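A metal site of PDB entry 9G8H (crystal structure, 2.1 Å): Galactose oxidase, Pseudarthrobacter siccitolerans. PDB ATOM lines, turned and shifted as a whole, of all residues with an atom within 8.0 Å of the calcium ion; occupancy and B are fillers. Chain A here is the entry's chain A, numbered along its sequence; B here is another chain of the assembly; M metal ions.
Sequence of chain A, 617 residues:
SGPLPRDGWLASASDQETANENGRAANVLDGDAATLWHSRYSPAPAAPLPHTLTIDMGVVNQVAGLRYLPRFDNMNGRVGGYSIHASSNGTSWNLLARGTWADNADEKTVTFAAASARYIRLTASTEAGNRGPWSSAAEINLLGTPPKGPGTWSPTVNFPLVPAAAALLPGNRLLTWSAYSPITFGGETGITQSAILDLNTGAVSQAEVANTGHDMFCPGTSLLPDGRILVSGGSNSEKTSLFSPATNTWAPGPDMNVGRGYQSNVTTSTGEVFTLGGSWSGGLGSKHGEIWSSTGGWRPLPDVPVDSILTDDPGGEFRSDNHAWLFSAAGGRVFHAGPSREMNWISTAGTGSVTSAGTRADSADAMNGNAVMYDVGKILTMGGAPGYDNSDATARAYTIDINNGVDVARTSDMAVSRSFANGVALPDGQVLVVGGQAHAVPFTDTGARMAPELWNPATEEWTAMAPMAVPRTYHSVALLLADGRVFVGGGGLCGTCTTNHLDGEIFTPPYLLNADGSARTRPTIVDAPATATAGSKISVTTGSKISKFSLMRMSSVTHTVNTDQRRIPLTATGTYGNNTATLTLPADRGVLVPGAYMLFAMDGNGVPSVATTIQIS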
ATOM      1  N   ARG A   6     -19.919  22.206  15.769  1.00  0.00           N
ATOM      2  CA  ARG A   6     -18.537  22.381  16.194  1.00  0.00           C
ATOM      3  C   ARG A   6     -17.781  23.397  15.325  1.00  0.00           C
ATOM      4  O   ARG A   6     -16.575  23.544  15.486  1.00  0.00           O
ATOM      5  CB  ARG A   6     -17.797  21.038  16.205  1.00  0.00           C
ATOM      6  CG  ARG A   6     -18.516  19.950  16.991  1.00  0.00           C
ATOM      7  CD  ARG A   6     -17.722  18.660  17.147  1.00  0.00           C
ATOM      8  NE  ARG A   6     -17.541  17.939  15.905  1.00  0.00           N
ATOM      9  CZ  ARG A   6     -16.633  16.985  15.715  1.00  0.00           C
ATOM     10  NH1 ARG A   6     -15.940  16.524  16.743  1.00  0.00           N
ATOM     11  NH2 ARG A   6     -16.413  16.505  14.498  1.00  0.00           N
ATOM     12  N   ARG A  24      -2.329  14.974  16.612  1.00  0.00           N
ATOM     13  CA  ARG A  24      -2.646  16.335  17.051  1.00  0.00           C
ATOM     14  C   ARG A  24      -4.039  16.406  17.668  1.00  0.00           C
ATOM     15  O   ARG A  24      -4.971  15.743  17.209  1.00  0.00           O
ATOM     16  CB  ARG A  24      -2.487  17.337  15.916  1.00  0.00           C
ATOM     17  CG  ARG A  24      -1.091  17.347  15.328  1.00  0.00           C
ATOM     18  CD  ARG A  24      -1.010  18.347  14.184  1.00  0.00           C
ATOM     19  NE  ARG A  24       0.372  18.640  13.828  1.00  0.00           N
ATOM     20  CZ  ARG A  24       1.108  17.907  13.005  1.00  0.00           C
ATOM     21  NH1 ARG A  24       0.616  16.805  12.452  1.00  0.00           N
ATOM     22  NH2 ARG A  24       2.339  18.304  12.729  1.00  0.00           N
ATOM     23  N   ALA A  25      -4.139  17.230  18.732  1.00  0.00           N
ATOM     24  CA  ALA A  25      -5.395  17.544  19.408  1.00  0.00           C
ATOM     25  C   ALA A  25      -6.535  17.817  18.412  1.00  0.00           C
ATOM     26  O   ALA A  25      -7.655  17.359  18.637  1.00  0.00           O
ATOM     27  CB  ALA A  25      -5.187  18.698  20.340  1.00  0.00           C
ATOM     28  N   ALA A  26      -6.234  18.514  17.292  1.00  0.00           N
ATOM     29  CA  ALA A  26      -7.205  18.996  16.324  1.00  0.00           C
ATOM     30  C   ALA A  26      -7.947  17.852  15.609  1.00  0.00           C
ATOM     31  O   ALA A  26      -8.990  18.081  14.991  1.00  0.00           O
ATOM     32  CB  ALA A  26      -6.544  19.929  15.342  1.00  0.00           C
ATOM     33  N   ASN A  27      -7.412  16.633  15.705  1.00  0.00           N
ATOM     34  CA  ASN A  27      -7.942  15.450  15.038  1.00  0.00           C
ATOM     35  C   ASN A  27      -9.226  14.941  15.716  1.00  0.00           C
ATOM     36  O   ASN A  27      -9.827  13.996  15.218  1.00  0.00           O
ATOM     37  CB  ASN A  27      -6.948  14.289  15.007  1.00  0.00           C
ATOM     38  CG  ASN A  27      -5.696  14.551  14.189  1.00  0.00           C
ATOM     39  OD1 ASN A  27      -5.653  15.494  13.408  1.00  0.00           O
ATOM     40  ND2 ASN A  27      -4.679  13.721  14.370  1.00  0.00           N
ATOM     41  N   VAL A  28      -9.602  15.515  16.880  1.00  0.00           N
ATOM     42  CA  VAL A  28     -10.794  15.070  17.591  1.00  0.00           C
ATOM     43  C   VAL A  28     -12.012  15.838  17.056  1.00  0.00           C
ATOM     44  O   VAL A  28     -13.134  15.497  17.419  1.00  0.00           O
ATOM     45  CB  VAL A  28     -10.715  15.270  19.120  1.00  0.00           C
ATOM     46  CG1 VAL A  28      -9.604  14.483  19.806  1.00  0.00           C
ATOM     47  CG2 VAL A  28     -10.664  16.743  19.518  1.00  0.00           C
ATOM     48  N   LEU A  29     -11.761  16.860  16.222  1.00  0.00           N
ATOM     49  CA  LEU A  29     -12.811  17.762  15.774  1.00  0.00           C
ATOM     50  C   LEU A  29     -13.108  17.622  14.272  1.00  0.00           C
ATOM     51  O   LEU A  29     -14.072  18.194  13.798  1.00  0.00           O
ATOM     52  CB  LEU A  29     -12.410  19.218  16.039  1.00  0.00           C
ATOM     53  CG  LEU A  29     -12.131  19.643  17.478  1.00  0.00           C
ATOM     54  CD1 LEU A  29     -11.839  21.130  17.509  1.00  0.00           C
ATOM     55  CD2 LEU A  29     -13.313  19.302  18.386  1.00  0.00           C
ATOM     56  N   ASP A  30     -12.302  16.854  13.527  1.00  0.00           N
ATOM     57  CA  ASP A  30     -12.382  16.847  12.076  1.00  0.00           C
ATOM     58  C   ASP A  30     -13.542  15.966  11.559  1.00  0.00           C
ATOM     59  O   ASP A  30     -13.847  15.994  10.372  1.00  0.00           O
ATOM     60  CB  ASP A  30     -11.029  16.445  11.459  1.00  0.00           C
ATOM     61  CG  ASP A  30     -10.516  15.046  11.776  1.00  0.00           C
ATOM     62  OD1 ASP A  30     -11.264  14.251  12.410  1.00  0.00           O
ATOM     63  OD2 ASP A  30      -9.367  14.748  11.384  1.00  0.00           O
ATOM     64  N   GLY A  31     -14.154  15.146  12.429  1.00  0.00           N
ATOM     65  CA  GLY A  31     -15.201  14.246  11.966  1.00  0.00           C
ATOM     66  C   GLY A  31     -14.720  12.906  11.395  1.00  0.00           C
ATOM     67  O   GLY A  31     -15.548  12.028  11.131  1.00  0.00           O
ATOM     68  N   ASP A  32     -13.415  12.719  11.229  1.00  0.00           N
ATOM     69  CA  ASP A  32     -12.843  11.480  10.708  1.00  0.00           C
ATOM     70  C   ASP A  32     -12.553  10.468  11.848  1.00  0.00           C
ATOM     71  O   ASP A  32     -11.781  10.732  12.782  1.00  0.00           O
ATOM     72  CB  ASP A  32     -11.633  11.811   9.826  1.00  0.00           C
ATOM     73  CG  ASP A  32     -10.952  10.636   9.125  1.00  0.00           C
ATOM     74  OD1 ASP A  32     -11.217   9.496   9.505  1.00  0.00           O
ATOM     75  OD2 ASP A  32     -10.181  10.876   8.187  1.00  0.00           O
ATOM     76  N   ALA A  33     -13.117   9.261  11.718  1.00  0.00           N
ATOM     77  CA  ALA A  33     -12.980   8.195  12.713  1.00  0.00           C
ATOM     78  C   ALA A  33     -11.553   7.613  12.759  1.00  0.00           C
ATOM     79  O   ALA A  33     -11.145   7.051  13.790  1.00  0.00           O
ATOM     80  CB  ALA A  33     -14.000   7.115  12.436  1.00  0.00           C
ATOM     81  N   ALA A  34     -10.826   7.769  11.637  1.00  0.00           N
ATOM     82  CA  ALA A  34      -9.457   7.297  11.442  1.00  0.00           C
ATOM     83  C   ALA A  34      -8.396   8.242  12.028  1.00  0.00           C
ATOM     84  O   ALA A  34      -7.290   7.783  12.279  1.00  0.00           O
ATOM     85  CB  ALA A  34      -9.205   6.985   9.987  1.00  0.00           C
ATOM     86  N   THR A  35      -8.685   9.538  12.262  1.00  0.00           N
ATOM     87  CA  THR A  35      -7.683  10.466  12.812  1.00  0.00           C
ATOM     88  C   THR A  35      -7.868  10.664  14.317  1.00  0.00           C
ATOM     89  O   THR A  35      -8.986  10.904  14.789  1.00  0.00           O
ATOM     90  CB  THR A  35      -7.631  11.812  12.061  1.00  0.00           C
ATOM     91  OG1 THR A  35      -8.886  12.488  12.070  1.00  0.00           O
ATOM     92  CG2 THR A  35      -7.143  11.693  10.631  1.00  0.00           C
ATOM     93  N   LEU A  36      -6.746  10.644  15.057  1.00  0.00           N
ATOM     94  CA  LEU A  36      -6.737  10.602  16.518  1.00  0.00           C
ATOM     95  C   LEU A  36      -5.941  11.759  17.105  1.00  0.00           C
ATOM     96  O   LEU A  36      -4.967  12.227  16.496  1.00  0.00           O
ATOM     97  CB  LEU A  36      -6.036   9.327  17.017  1.00  0.00           C
ATOM     98  CG  LEU A  36      -6.358   7.995  16.359  1.00  0.00           C
ATOM     99  CD1 LEU A  36      -5.546   6.887  17.020  1.00  0.00           C
ATOM    100  CD2 LEU A  36      -7.853   7.689  16.452  1.00  0.00           C
ATOM    101  N   TRP A  37      -6.347  12.155  18.320  1.00  0.00           N
ATOM    102  CA  TRP A  37      -5.434  12.729  19.289  1.00  0.00           C
ATOM    103  C   TRP A  37      -4.800  11.597  20.082  1.00  0.00           C
ATOM    104  O   TRP A  37      -5.507  10.745  20.634  1.00  0.00           O
ATOM    105  CB  TRP A  37      -6.157  13.694  20.250  1.00  0.00           C
ATOM    106  CG  TRP A  37      -5.318  14.017  21.453  1.00  0.00           C
ATOM    107  CD1 TRP A  37      -4.118  14.680  21.466  1.00  0.00           C
ATOM    108  CD2 TRP A  37      -5.602  13.690  22.837  1.00  0.00           C
ATOM    109  NE1 TRP A  37      -3.649  14.802  22.751  1.00  0.00           N
ATOM    110  CE2 TRP A  37      -4.534  14.206  23.622  1.00  0.00           C
ATOM    111  CE3 TRP A  37      -6.652  13.023  23.492  1.00  0.00           C
ATOM    112  CZ2 TRP A  37      -4.486  14.077  25.007  1.00  0.00           C
ATOM    113  CZ3 TRP A  37      -6.619  12.907  24.869  1.00  0.00           C
ATOM    114  CH2 TRP A  37      -5.548  13.431  25.608  1.00  0.00           C
ATOM    115  N   LEU A  69     -15.425   9.321  21.343  1.00  0.00           N
ATOM    116  CA  LEU A  69     -15.309   8.241  20.372  1.00  0.00           C
ATOM    117  C   LEU A  69     -13.876   7.705  20.353  1.00  0.00           C
ATOM    118  O   LEU A  69     -12.931   8.408  19.988  1.00  0.00           O
ATOM    119  CB  LEU A  69     -15.814   8.683  18.988  1.00  0.00           C
ATOM    120  CG  LEU A  69     -15.662   7.654  17.863  1.00  0.00           C
ATOM    121  CD1 LEU A  69     -16.701   6.542  17.938  1.00  0.00           C
ATOM    122  CD2 LEU A  69     -15.680   8.321  16.480  1.00  0.00           C
ATOM    123  N   ALA A 137      -8.128   9.746  21.391  1.00  0.00           N
ATOM    124  CA  ALA A 137      -9.525   9.965  21.034  1.00  0.00           C
ATOM    125  C   ALA A 137      -9.620  10.220  19.538  1.00  0.00           C
ATOM    126  O   ALA A 137      -8.756  10.905  18.965  1.00  0.00           O
ATOM    127  CB  ALA A 137     -10.111  11.111  21.834  1.00  0.00           C
ATOM    128  N   ALA A 138     -10.664   9.646  18.902  1.00  0.00           N
ATOM    129  CA  ALA A 138     -10.928   9.860  17.491  1.00  0.00           C
ATOM    130  C   ALA A 138     -11.815  11.087  17.301  1.00  0.00           C
ATOM    131  O   ALA A 138     -11.567  11.872  16.377  1.00  0.00           O
ATOM    132  CB  ALA A 138     -11.529   8.620  16.845  1.00  0.00           C
ATOM    133  N   GLU A 139     -12.838  11.246  18.151  1.00  0.00           N
ATOM    134  CA  GLU A 139     -13.782  12.341  18.045  1.00  0.00           C
ATOM    135  C   GLU A 139     -14.238  12.772  19.445  1.00  0.00           C
ATOM    136  O   GLU A 139     -14.345  11.923  20.316  1.00  0.00           O
ATOM    137  CB  GLU A 139     -14.983  11.934  17.173  1.00  0.00           C
ATOM    138  CG  GLU A 139     -14.700  11.913  15.666  1.00  0.00           C
ATOM    139  CD  GLU A 139     -14.220  13.215  15.035  1.00  0.00           C
ATOM    140  OE1 GLU A 139     -14.973  14.231  15.102  1.00  0.00           O
ATOM    141  OE2 GLU A 139     -13.082  13.217  14.504  1.00  0.00           O
ATOM    142  N   ILE A 140     -14.487  14.078  19.625  1.00  0.00           N
ATOM    143  CA  ILE A 140     -15.166  14.602  20.800  1.00  0.00           C
ATOM    144  C   ILE A 140     -16.340  15.473  20.350  1.00  0.00           C
ATOM    145  O   ILE A 140     -16.145  16.502  19.684  1.00  0.00           O
ATOM    146  CB  ILE A 140     -14.229  15.439  21.699  1.00  0.00           C
ATOM    147  CG1 ILE A 140     -13.016  14.651  22.188  1.00  0.00           C
ATOM    148  CG2 ILE A 140     -15.003  16.102  22.850  1.00  0.00           C
ATOM    149  CD1 ILE A 140     -13.328  13.615  23.259  1.00  0.00           C
ATOM    150  N   SER B   1     -20.239  10.693  11.491  1.00  0.00           N
ATOM    151  CA  SER B   1     -18.795  10.865  11.173  1.00  0.00           C
ATOM    152  C   SER B   1     -18.490  10.246   9.810  1.00  0.00           C
ATOM    153  O   SER B   1     -19.390   9.781   9.126  1.00  0.00           O
ATOM    154  CB  SER B   1     -17.911  10.313  12.265  1.00  0.00           C
ATOM    155  OG  SER B   1     -18.237   8.964  12.566  1.00  0.00           O
ATOM    156  N   HIS B   2     -17.225  10.297   9.421  1.00  0.00           N
ATOM    157  CA  HIS B   2     -16.724   9.604   8.245  1.00  0.00           C
ATOM    158  C   HIS B   2     -15.352   9.019   8.586  1.00  0.00           C
ATOM    159  O   HIS B   2     -14.894   9.133   9.730  1.00  0.00           O
ATOM    160  CB  HIS B   2     -16.659  10.558   7.053  1.00  0.00           C
ATOM    161  CG  HIS B   2     -15.758  11.711   7.304  1.00  0.00           C
ATOM    162  ND1 HIS B   2     -16.099  12.770   8.128  1.00  0.00           N
ATOM    163  CD2 HIS B   2     -14.541  11.983   6.843  1.00  0.00           C
ATOM    164  CE1 HIS B   2     -15.106  13.641   8.155  1.00  0.00           C
ATOM    165  NE2 HIS B   2     -14.144  13.178   7.383  1.00  0.00           N
HETATM  166 CA    CA M   1     -10.950  12.466  14.104  1.00  0.00          CA
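ND2 of Asn 27 is in hydrogen-bond range of O of Leu 36. The backbone NH of Arg 24 sits close to the side-chain amide nitrogen of Asn 27 (3.5 Å). N of Gly 31 is in hydrogen-bond range of OE1 of Glu 139 (2.9 Å). The backbone carbonyl oxygen (O) of Glu 139 lies within hydrogen-bond range of the backbone NH (N) of Leu 69 (3.0 Å). The side-chain carboxylate (OE1) of Glu 139 lies within salt-bridge range of the guanidinium group (NH2) of Arg 6 (2.8 Å). N of Ala 34 sits at hydrogen-bond distance from OD1 of Asp 32, at 2.8 Å. The backbone NH (N) of Ala 138 lies within hydrogen-bond range of the backbone carbonyl oxygen (O) of Leu 69.
Within 4 Å of the calcium ion: Asn 27, Asp 30, Asp 32, Thr 35, Ala 138 and Glu 139.
O of Asn 27 binds the calcium ion (2.2 Å). The calcium ion is bound by the side-chain carboxylate (OE2) of Glu 139 (2.3 Å). The calcium ion is bound by O of Asp 32, 2.3 Å away. The calcium ion is bound by the backbone carbonyl oxygen (O) of Ala 138, at 2.4 Å. The calcium ion is bound by OD1 of Asp 30. The calcium ion is bound by the backbone carbonyl oxygen (O) of Thr 35. OG1 of Thr 35 binds the calcium ion (2.9 Å). The calcium ion has seven donor atoms within binding distance.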
